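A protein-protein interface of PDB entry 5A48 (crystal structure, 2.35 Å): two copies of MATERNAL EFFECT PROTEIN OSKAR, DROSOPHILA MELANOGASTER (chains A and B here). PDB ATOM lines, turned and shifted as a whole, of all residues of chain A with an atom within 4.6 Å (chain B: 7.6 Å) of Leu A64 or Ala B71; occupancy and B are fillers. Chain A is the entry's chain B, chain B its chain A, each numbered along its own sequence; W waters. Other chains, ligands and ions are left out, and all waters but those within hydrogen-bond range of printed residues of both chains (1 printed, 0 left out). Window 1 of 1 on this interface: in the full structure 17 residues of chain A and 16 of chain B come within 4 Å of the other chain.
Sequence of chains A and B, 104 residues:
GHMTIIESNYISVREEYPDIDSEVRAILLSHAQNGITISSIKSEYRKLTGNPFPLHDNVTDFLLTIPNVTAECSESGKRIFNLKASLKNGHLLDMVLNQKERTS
CG2 of Thr A60 touches CD1 of Leu B64, 3.9 Å away.
Leu A64 touches Thr B60 (CD1 to CG2, 3.9 Å).
CD1 of Leu A64 touches CB of Ala B71 (3.8 Å).
Thr A65 touches Cys B73 (C to SG, 3.9 Å).
Thr A65 touches Arg B79.
Val A69 touches Ala B71.
CA of Glu B72 touches O of Val A69 (3.4 Å).
Thr A70 touches Ala B71.
CG2 of Thr A70 touches CB of Glu B72 (3.7 Å).
CA of Thr B70 touches O of Ala A71 (3.2 Å).
The backbone NH of Cys B73 lies within hydrogen-bond range of the backbone carbonyl oxygen of Val A69, at 3.0 Å.
The backbone NH (N) of Ala A71 is in hydrogen-bond range of the backbone carbonyl oxygen (O) of Ala B71 (2.6 Å).
The side-chain sulfur of Cys B73 sits close to the backbone carbonyl oxygen of Ile A66, 3.7 Å away.
The guanidinium group (NH2) of Arg B79 is in hydrogen-bond range of the backbone carbonyl oxygen (O) of Leu A64 (3.2 Å).
The guanidinium group of Arg B79 lies within salt-bridge range of the side-chain carboxylate of Asp A61, at 3.0 Å.
SG of Cys B73 is in hydrogen-bond range of O of Leu A64 (3.3 Å).
Of the printed residues of chain B, Leu A64 touches Thr B60, Ala B71, Cys B73 and Arg B79.
Printed residues of chain A within 4 Å of Ala B71: Leu A64 (3.8 Å), Val A69 (3.995 Å), Thr A70 (3.2 Å) and Ala A71 (2.6 Å).
Of the printed residues of chain B, Val A69 touches Ala B71 (3.995 Å), Glu B72 (3.4 Å) and Cys B73 (3.0 Å).
Of the printed residues of chain A, Thr B70 touches Ala A71.
Of the printed residues of chain B, Thr A65 touches Cys B73 (3.9 Å) and Arg B79 (3.9 Å).
Of the printed residues of chain B, Thr A70 touches Ala B71 and Glu B72.
Of the printed residues of chain A, Cys B73 touches Leu A64, Thr A65, Ile A66 and Val A69.
The nearest printed residue of chain B that does not touch Thr A60 is Thr B60 (4.2 Å).
Water W1 lies within hydrogen-bond range of O of Leu A64 (2.6 Å), O of Gly B77 (2.7 Å), NE of Arg B79 (3.3 Å) and SG of Cys B73 (3.3 Å).
Thr A60 touches Leu B64, and with the chains exchanged Leu A64 touches Thr B60.
Val A69 touches Ala B71, but with the chains exchanged Ala A71 does not touch Val B69 (4.2 Å).
Thr A70 touches Ala B71, and with the chains exchanged Ala A71 touches Thr B70.
Ala A71 touches its own counterpart, Ala B71.
Positions printed for both chains: 60, 61, 63, 64, 69, 70 and 71.
Of the 16 pairs that touch across the chains among the printed residues, 5 have their exchanged pair printed and touching as well.
The backbone carbonyl oxygen (O) of Ile B80 sits at hydrogen-bond distance from the backbone NH (N) of Glu B72, 2.9 Å away.
The side-chain hydroxyl of Thr B60 lies within hydrogen-bond range of the guanidinium group of Arg B79 (3.1 Å).
The backbone carbonyl oxygen of Asn B82 lies within hydrogen-bond range of the backbone NH of Thr B70, at 2.9 Å.
Along chain A the printed residues that touch a printed residue of chain B span positions 60 to 71.
Along chain B the printed residues that touch a printed residue of chain A span positions 60 to 79.
Among the printed residues, 16 pairs touch across the chains.
Among the printed residues, Asp or Glu carboxylates within 4 Å of a Lys or Arg side-chain nitrogen of the other chain: Asp A61 with Arg B79 (3.0 Å).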
ATOM      1  N   THR A  60      25.315 -20.251 -31.175  1.00  0.00           N
ATOM      2  CA  THR A  60      25.258 -21.604 -30.623  1.00  0.00           C
ATOM      3  C   THR A  60      25.192 -21.596 -29.096  1.00  0.00           C
ATOM      4  O   THR A  60      24.358 -22.281 -28.501  1.00  0.00           O
ATOM      5  CB  THR A  60      26.480 -22.440 -31.056  1.00  0.00           C
ATOM      6  OG1 THR A  60      26.551 -22.487 -32.487  1.00  0.00           O
ATOM      7  CG2 THR A  60      26.386 -23.857 -30.509  1.00  0.00           C
ATOM      8  N   ASP A  61      26.070 -20.820 -28.469  1.00  0.00           N
ATOM      9  CA  ASP A  61      26.097 -20.724 -27.012  1.00  0.00           C
ATOM     10  C   ASP A  61      24.822 -20.090 -26.459  1.00  0.00           C
ATOM     11  O   ASP A  61      24.301 -20.532 -25.438  1.00  0.00           O
ATOM     12  CB  ASP A  61      27.333 -19.952 -26.533  1.00  0.00           C
ATOM     13  CG  ASP A  61      27.304 -19.665 -25.042  1.00  0.00           C
ATOM     14  OD1 ASP A  61      27.463 -20.617 -24.248  1.00  0.00           O
ATOM     15  OD2 ASP A  61      27.136 -18.487 -24.667  1.00  0.00           O
ATOM     16  N   PHE A  62      24.322 -19.061 -27.138  1.00  0.00           N
ATOM     17  CA  PHE A  62      23.097 -18.389 -26.710  1.00  0.00           C
ATOM     18  C   PHE A  62      21.898 -19.328 -26.785  1.00  0.00           C
ATOM     19  O   PHE A  62      21.077 -19.380 -25.869  1.00  0.00           O
ATOM     20  CB  PHE A  62      22.825 -17.133 -27.546  1.00  0.00           C
ATOM     21  CG  PHE A  62      21.488 -16.504 -27.263  1.00  0.00           C
ATOM     22  CD1 PHE A  62      21.308 -15.710 -26.144  1.00  0.00           C
ATOM     23  CD2 PHE A  62      20.410 -16.718 -28.107  1.00  0.00           C
ATOM     24  CE1 PHE A  62      20.080 -15.137 -25.876  1.00  0.00           C
ATOM     25  CE2 PHE A  62      19.180 -16.145 -27.840  1.00  0.00           C
ATOM     26  CZ  PHE A  62      19.015 -15.356 -26.724  1.00  0.00           C
ATOM     27  N   LEU A  63      21.804 -20.060 -27.890  1.00  0.00           N
ATOM     28  CA  LEU A  63      20.709 -20.995 -28.105  1.00  0.00           C
ATOM     29  C   LEU A  63      20.739 -22.112 -27.069  1.00  0.00           C
ATOM     30  O   LEU A  63      19.696 -22.602 -26.640  1.00  0.00           O
ATOM     31  CB  LEU A  63      20.780 -21.583 -29.515  1.00  0.00           C
ATOM     32  CG  LEU A  63      20.557 -20.605 -30.672  1.00  0.00           C
ATOM     33  CD1 LEU A  63      20.735 -21.305 -32.015  1.00  0.00           C
ATOM     34  CD2 LEU A  63      19.183 -19.964 -30.571  1.00  0.00           C
ATOM     35  N   LEU A  64      21.944 -22.503 -26.664  1.00  0.00           N
ATOM     36  CA  LEU A  64      22.109 -23.550 -25.663  1.00  0.00           C
ATOM     37  C   LEU A  64      22.046 -23.003 -24.235  1.00  0.00           C
ATOM     38  O   LEU A  64      22.471 -23.666 -23.288  1.00  0.00           O
ATOM     39  CB  LEU A  64      23.404 -24.336 -25.902  1.00  0.00           C
ATOM     40  CG  LEU A  64      23.429 -25.196 -27.172  1.00  0.00           C
ATOM     41  CD1 LEU A  64      24.750 -25.948 -27.324  1.00  0.00           C
ATOM     42  CD2 LEU A  64      22.254 -26.164 -27.185  1.00  0.00           C
ATOM     43  N   THR A  65      21.518 -21.790 -24.088  1.00  0.00           N
ATOM     44  CA  THR A  65      21.172 -21.259 -22.772  1.00  0.00           C
ATOM     45  C   THR A  65      19.657 -21.286 -22.623  1.00  0.00           C
ATOM     46  O   THR A  65      19.104 -20.845 -21.613  1.00  0.00           O
ATOM     47  CB  THR A  65      21.689 -19.823 -22.559  1.00  0.00           C
ATOM     48  OG1 THR A  65      21.179 -18.968 -23.591  1.00  0.00           O
ATOM     49  CG2 THR A  65      23.209 -19.794 -22.578  1.00  0.00           C
ATOM     50  N   ILE A  66      18.996 -21.804 -23.653  1.00  0.00           N
ATOM     51  CA  ILE A  66      17.558 -22.021 -23.625  1.00  0.00           C
ATOM     52  C   ILE A  66      17.294 -23.498 -23.374  1.00  0.00           C
ATOM     53  O   ILE A  66      17.669 -24.342 -24.185  1.00  0.00           O
ATOM     54  CB  ILE A  66      16.906 -21.610 -24.951  1.00  0.00           C
ATOM     55  CG1 ILE A  66      17.230 -20.149 -25.274  1.00  0.00           C
ATOM     56  CG2 ILE A  66      15.403 -21.834 -24.900  1.00  0.00           C
ATOM     57  CD1 ILE A  66      16.729 -19.696 -26.628  1.00  0.00           C
ATOM     58  N   VAL A  69      16.737 -26.992 -25.694  1.00  0.00           N
ATOM     59  CA  VAL A  69      17.315 -26.794 -27.018  1.00  0.00           C
ATOM     60  C   VAL A  69      18.461 -27.773 -27.230  1.00  0.00           C
ATOM     61  O   VAL A  69      19.363 -27.882 -26.399  1.00  0.00           O
ATOM     62  CB  VAL A  69      17.835 -25.352 -27.224  1.00  0.00           C
ATOM     63  CG1 VAL A  69      18.665 -25.254 -28.500  1.00  0.00           C
ATOM     64  CG2 VAL A  69      16.679 -24.369 -27.258  1.00  0.00           C
ATOM     65  N   THR A  70      18.412 -28.493 -28.343  1.00  0.00           N
ATOM     66  CA  THR A  70      19.476 -29.420 -28.690  1.00  0.00           C
ATOM     67  C   THR A  70      20.174 -28.973 -29.964  1.00  0.00           C
ATOM     68  O   THR A  70      19.568 -28.341 -30.830  1.00  0.00           O
ATOM     69  CB  THR A  70      18.941 -30.845 -28.902  1.00  0.00           C
ATOM     70  OG1 THR A  70      18.060 -30.860 -30.031  1.00  0.00           O
ATOM     71  CG2 THR A  70      18.195 -31.326 -27.667  1.00  0.00           C
ATOM     72  N   ALA A  71      21.456 -29.297 -30.063  1.00  0.00           N
ATOM     73  CA  ALA A  71      22.219 -29.053 -31.277  1.00  0.00           C
ATOM     74  C   ALA A  71      22.964 -30.330 -31.634  1.00  0.00           C
ATOM     75  O   ALA A  71      23.258 -31.142 -30.760  1.00  0.00           O
ATOM     76  CB  ALA A  71      23.194 -27.906 -31.069  1.00  0.00           C
ATOM     77  N   THR B  60      32.327 -25.816 -26.721  1.00  0.00           N
ATOM     78  CA  THR B  60      31.070 -26.240 -27.329  1.00  0.00           C
ATOM     79  C   THR B  60      31.156 -26.247 -28.852  1.00  0.00           C
ATOM     80  O   THR B  60      30.785 -27.230 -29.497  1.00  0.00           O
ATOM     81  CB  THR B  60      29.910 -25.318 -26.900  1.00  0.00           C
ATOM     82  OG1 THR B  60      29.803 -25.310 -25.471  1.00  0.00           O
ATOM     83  CG2 THR B  60      28.597 -25.789 -27.504  1.00  0.00           C
ATOM     84  N   ASP B  61      31.661 -25.151 -29.412  1.00  0.00           N
ATOM     85  CA  ASP B  61      31.814 -25.018 -30.857  1.00  0.00           C
ATOM     86  C   ASP B  61      32.739 -26.083 -31.425  1.00  0.00           C
ATOM     87  O   ASP B  61      32.432 -26.691 -32.446  1.00  0.00           O
ATOM     88  CB  ASP B  61      32.326 -23.623 -31.227  1.00  0.00           C
ATOM     89  CG  ASP B  61      32.597 -23.473 -32.712  1.00  0.00           C
ATOM     90  OD1 ASP B  61      31.624 -23.433 -33.494  1.00  0.00           O
ATOM     91  OD2 ASP B  61      33.783 -23.385 -33.095  1.00  0.00           O
ATOM     92  N   LEU B  63      33.567 -29.050 -30.023  1.00  0.00           N
ATOM     93  CA  LEU B  63      32.927 -30.345 -29.826  1.00  0.00           C
ATOM     94  C   LEU B  63      31.892 -30.613 -30.911  1.00  0.00           C
ATOM     95  O   LEU B  63      31.713 -31.748 -31.353  1.00  0.00           O
ATOM     96  CB  LEU B  63      32.266 -30.413 -28.448  1.00  0.00           C
ATOM     97  CG  LEU B  63      33.190 -30.442 -27.232  1.00  0.00           C
ATOM     98  CD1 LEU B  63      32.385 -30.474 -25.936  1.00  0.00           C
ATOM     99  CD2 LEU B  63      34.145 -31.625 -27.313  1.00  0.00           C
ATOM    100  N   LEU B  64      31.226 -29.550 -31.349  1.00  0.00           N
ATOM    101  CA  LEU B  64      30.163 -29.651 -32.343  1.00  0.00           C
ATOM    102  C   LEU B  64      30.669 -29.540 -33.784  1.00  0.00           C
ATOM    103  O   LEU B  64      29.879 -29.346 -34.709  1.00  0.00           O
ATOM    104  CB  LEU B  64      29.081 -28.601 -32.071  1.00  0.00           C
ATOM    105  CG  LEU B  64      28.190 -28.881 -30.860  1.00  0.00           C
ATOM    106  CD1 LEU B  64      27.339 -27.675 -30.514  1.00  0.00           C
ATOM    107  CD2 LEU B  64      27.310 -30.083 -31.136  1.00  0.00           C
ATOM    108  N   ASN B  68      28.291 -36.276 -35.527  1.00  0.00           N
ATOM    109  CA  ASN B  68      27.462 -37.089 -34.621  1.00  0.00           C
ATOM    110  C   ASN B  68      27.398 -36.619 -33.161  1.00  0.00           C
ATOM    111  O   ASN B  68      26.630 -37.166 -32.372  1.00  0.00           O
ATOM    112  CB  ASN B  68      27.835 -38.579 -34.689  1.00  0.00           C
ATOM    113  CG  ASN B  68      27.760 -39.138 -36.094  1.00  0.00           C
ATOM    114  OD1 ASN B  68      28.730 -39.699 -36.603  1.00  0.00           O
ATOM    115  ND2 ASN B  68      26.605 -38.989 -36.731  1.00  0.00           N
ATOM    116  N   VAL B  69      28.191 -35.613 -32.806  1.00  0.00           N
ATOM    117  CA  VAL B  69      28.154 -35.062 -31.453  1.00  0.00           C
ATOM    118  C   VAL B  69      26.927 -34.178 -31.234  1.00  0.00           C
ATOM    119  O   VAL B  69      26.637 -33.291 -32.040  1.00  0.00           O
ATOM    120  CB  VAL B  69      29.430 -34.253 -31.134  1.00  0.00           C
ATOM    121  CG1 VAL B  69      29.289 -33.525 -29.802  1.00  0.00           C
ATOM    122  CG2 VAL B  69      30.649 -35.166 -31.126  1.00  0.00           C
ATOM    123  N   THR B  70      26.212 -34.426 -30.141  1.00  0.00           N
ATOM    124  CA  THR B  70      25.036 -33.637 -29.791  1.00  0.00           C
ATOM    125  C   THR B  70      25.278 -32.827 -28.526  1.00  0.00           C
ATOM    126  O   THR B  70      26.090 -33.201 -27.680  1.00  0.00           O
ATOM    127  CB  THR B  70      23.803 -34.530 -29.565  1.00  0.00           C
ATOM    128  OG1 THR B  70      24.018 -35.363 -28.419  1.00  0.00           O
ATOM    129  CG2 THR B  70      23.548 -35.401 -30.778  1.00  0.00           C
ATOM    130  N   ALA B  71      24.570 -31.711 -28.410  1.00  0.00           N
ATOM    131  CA  ALA B  71      24.611 -30.904 -27.200  1.00  0.00           C
ATOM    132  C   ALA B  71      23.201 -30.452 -26.861  1.00  0.00           C
ATOM    133  O   ALA B  71      22.456 -30.025 -27.741  1.00  0.00           O
ATOM    134  CB  ALA B  71      25.522 -29.707 -27.386  1.00  0.00           C
ATOM    135  N   GLU B  72      22.834 -30.553 -25.589  1.00  0.00           N
ATOM    136  CA  GLU B  72      21.503 -30.156 -25.159  1.00  0.00           C
ATOM    137  C   GLU B  72      21.592 -29.307 -23.903  1.00  0.00           C
ATOM    138  O   GLU B  72      22.438 -29.540 -23.041  1.00  0.00           O
ATOM    139  CB  GLU B  72      20.628 -31.386 -24.906  1.00  0.00           C
ATOM    140  CG  GLU B  72      21.117 -32.285 -23.781  1.00  0.00           C
ATOM    141  CD  GLU B  72      20.231 -33.500 -23.573  1.00  0.00           C
ATOM    142  OE1 GLU B  72      19.067 -33.327 -23.152  1.00  0.00           O
ATOM    143  OE2 GLU B  72      20.704 -34.629 -23.822  1.00  0.00           O
ATOM    144  N   CYS B  73      20.730 -28.303 -23.812  1.00  0.00           N
ATOM    145  CA  CYS B  73      20.636 -27.510 -22.600  1.00  0.00           C
ATOM    146  C   CYS B  73      19.595 -28.155 -21.705  1.00  0.00           C
ATOM    147  O   CYS B  73      18.430 -28.279 -22.087  1.00  0.00           O
ATOM    148  CB  CYS B  73      20.244 -26.072 -22.922  1.00  0.00           C
ATOM    149  SG  CYS B  73      20.094 -25.006 -21.466  1.00  0.00           S
ATOM    150  N   SER B  74      20.015 -28.593 -20.524  1.00  0.00           N
ATOM    151  CA  SER B  74      19.091 -29.211 -19.586  1.00  0.00           C
ATOM    152  C   SER B  74      18.219 -28.136 -18.957  1.00  0.00           C
ATOM    153  O   SER B  74      18.449 -26.944 -19.158  1.00  0.00           O
ATOM    154  CB  SER B  74      19.842 -29.984 -18.501  1.00  0.00           C
ATOM    155  OG  SER B  74      20.379 -29.106 -17.530  1.00  0.00           O
ATOM    156  N   GLY B  77      20.041 -25.688 -16.926  1.00  0.00           N
ATOM    157  CA  GLY B  77      20.953 -24.824 -17.653  1.00  0.00           C
ATOM    158  C   GLY B  77      22.256 -25.542 -17.942  1.00  0.00           C
ATOM    159  O   GLY B  77      23.097 -25.056 -18.699  1.00  0.00           O
ATOM    160  N   LYS B  78      22.415 -26.711 -17.328  1.00  0.00           N
ATOM    161  CA  LYS B  78      23.593 -27.543 -17.529  1.00  0.00           C
ATOM    162  C   LYS B  78      23.689 -27.998 -18.983  1.00  0.00           C
ATOM    163  O   LYS B  78      22.683 -28.349 -19.599  1.00  0.00           O
ATOM    164  CB  LYS B  78      23.547 -28.753 -16.590  1.00  0.00           C
ATOM    165  CG  LYS B  78      24.737 -29.691 -16.714  1.00  0.00           C
ATOM    166  CD  LYS B  78      24.697 -30.792 -15.662  1.00  0.00           C
ATOM    167  CE  LYS B  78      24.898 -30.229 -14.265  1.00  0.00           C
ATOM    168  NZ  LYS B  78      24.813 -31.284 -13.212  1.00  0.00           N
ATOM    169  N   ARG B  79      24.899 -27.984 -19.530  1.00  0.00           N
ATOM    170  CA  ARG B  79      25.100 -28.362 -20.925  1.00  0.00           C
ATOM    171  C   ARG B  79      25.616 -29.793 -21.049  1.00  0.00           C
ATOM    172  O   ARG B  79      26.705 -30.116 -20.572  1.00  0.00           O
ATOM    173  CB  ARG B  79      26.052 -27.383 -21.611  1.00  0.00           C
ATOM    174  CG  ARG B  79      26.106 -27.522 -23.120  1.00  0.00           C
ATOM    175  CD  ARG B  79      26.731 -26.291 -23.752  1.00  0.00           C
ATOM    176  NE  ARG B  79      25.956 -25.086 -23.463  1.00  0.00           N
ATOM    177  CZ  ARG B  79      26.271 -23.871 -23.900  1.00  0.00           C
ATOM    178  NH1 ARG B  79      27.347 -23.687 -24.651  1.00  0.00           N
ATOM    179  NH2 ARG B  79      25.505 -22.834 -23.584  1.00  0.00           N
ATOM    180  N   ILE B  80      24.826 -30.641 -21.698  1.00  0.00           N
ATOM    181  CA  ILE B  80      25.127 -32.064 -21.792  1.00  0.00           C
ATOM    182  C   ILE B  80      25.512 -32.465 -23.213  1.00  0.00           C
ATOM    183  O   ILE B  80      24.804 -32.145 -24.168  1.00  0.00           O
ATOM    184  CB  ILE B  80      23.915 -32.913 -21.349  1.00  0.00           C
ATOM    185  CG1 ILE B  80      23.395 -32.438 -19.991  1.00  0.00           C
ATOM    186  CG2 ILE B  80      24.279 -34.389 -21.303  1.00  0.00           C
ATOM    187  CD1 ILE B  80      24.393 -32.589 -18.867  1.00  0.00           C
ATOM    188  N   PHE B  81      26.635 -33.166 -23.347  1.00  0.00           N
ATOM    189  CA  PHE B  81      27.104 -33.637 -24.646  1.00  0.00           C
ATOM    190  C   PHE B  81      26.982 -35.157 -24.759  1.00  0.00           C
ATOM    191  O   PHE B  81      27.036 -35.870 -23.756  1.00  0.00           O
ATOM    192  CB  PHE B  81      28.551 -33.195 -24.896  1.00  0.00           C
ATOM    193  CG  PHE B  81      28.714 -31.704 -25.054  1.00  0.00           C
ATOM    194  CD1 PHE B  81      28.749 -30.873 -23.944  1.00  0.00           C
ATOM    195  CD2 PHE B  81      28.828 -31.133 -26.309  1.00  0.00           C
ATOM    196  CE1 PHE B  81      28.898 -29.504 -24.085  1.00  0.00           C
ATOM    197  CE2 PHE B  81      28.975 -29.764 -26.456  1.00  0.00           C
ATOM    198  CZ  PHE B  81      29.011 -28.949 -25.343  1.00  0.00           C
ATOM    199  N   ASN B  82      26.822 -35.644 -25.985  1.00  0.00           N
ATOM    200  CA  ASN B  82      26.615 -37.066 -26.229  1.00  0.00           C
ATOM    201  C   ASN B  82      26.808 -37.414 -27.701  1.00  0.00           C
ATOM    202  O   ASN B  82      27.244 -36.579 -28.497  1.00  0.00           O
ATOM    203  CB  ASN B  82      25.207 -37.468 -25.787  1.00  0.00           C
ATOM    204  CG  ASN B  82      25.140 -38.884 -25.245  1.00  0.00           C
ATOM    205  OD1 ASN B  82      25.881 -39.768 -25.675  1.00  0.00           O
ATOM    206  ND2 ASN B  82      24.245 -39.105 -24.289  1.00  0.00           N
ATOM    207  N   LEU B  83      26.482 -38.653 -28.055  1.00  0.00           N
ATOM    208  CA  LEU B  83      26.478 -39.088 -29.446  1.00  0.00           C
ATOM    209  C   LEU B  83      25.062 -39.438 -29.868  1.00  0.00           C
ATOM    210  O   LEU B  83      24.242 -39.839 -29.040  1.00  0.00           O
ATOM    211  CB  LEU B  83      27.378 -40.308 -29.643  1.00  0.00           C
ATOM    212  CG  LEU B  83      28.885 -40.071 -29.766  1.00  0.00           C
ATOM    213  CD1 LEU B  83      29.604 -41.393 -29.952  1.00  0.00           C
ATOM    214  CD2 LEU B  83      29.192 -39.133 -30.922  1.00  0.00           C
HETATM  215  O   HOH W   1      23.393 -25.154 -21.396  1.00  0.00           O
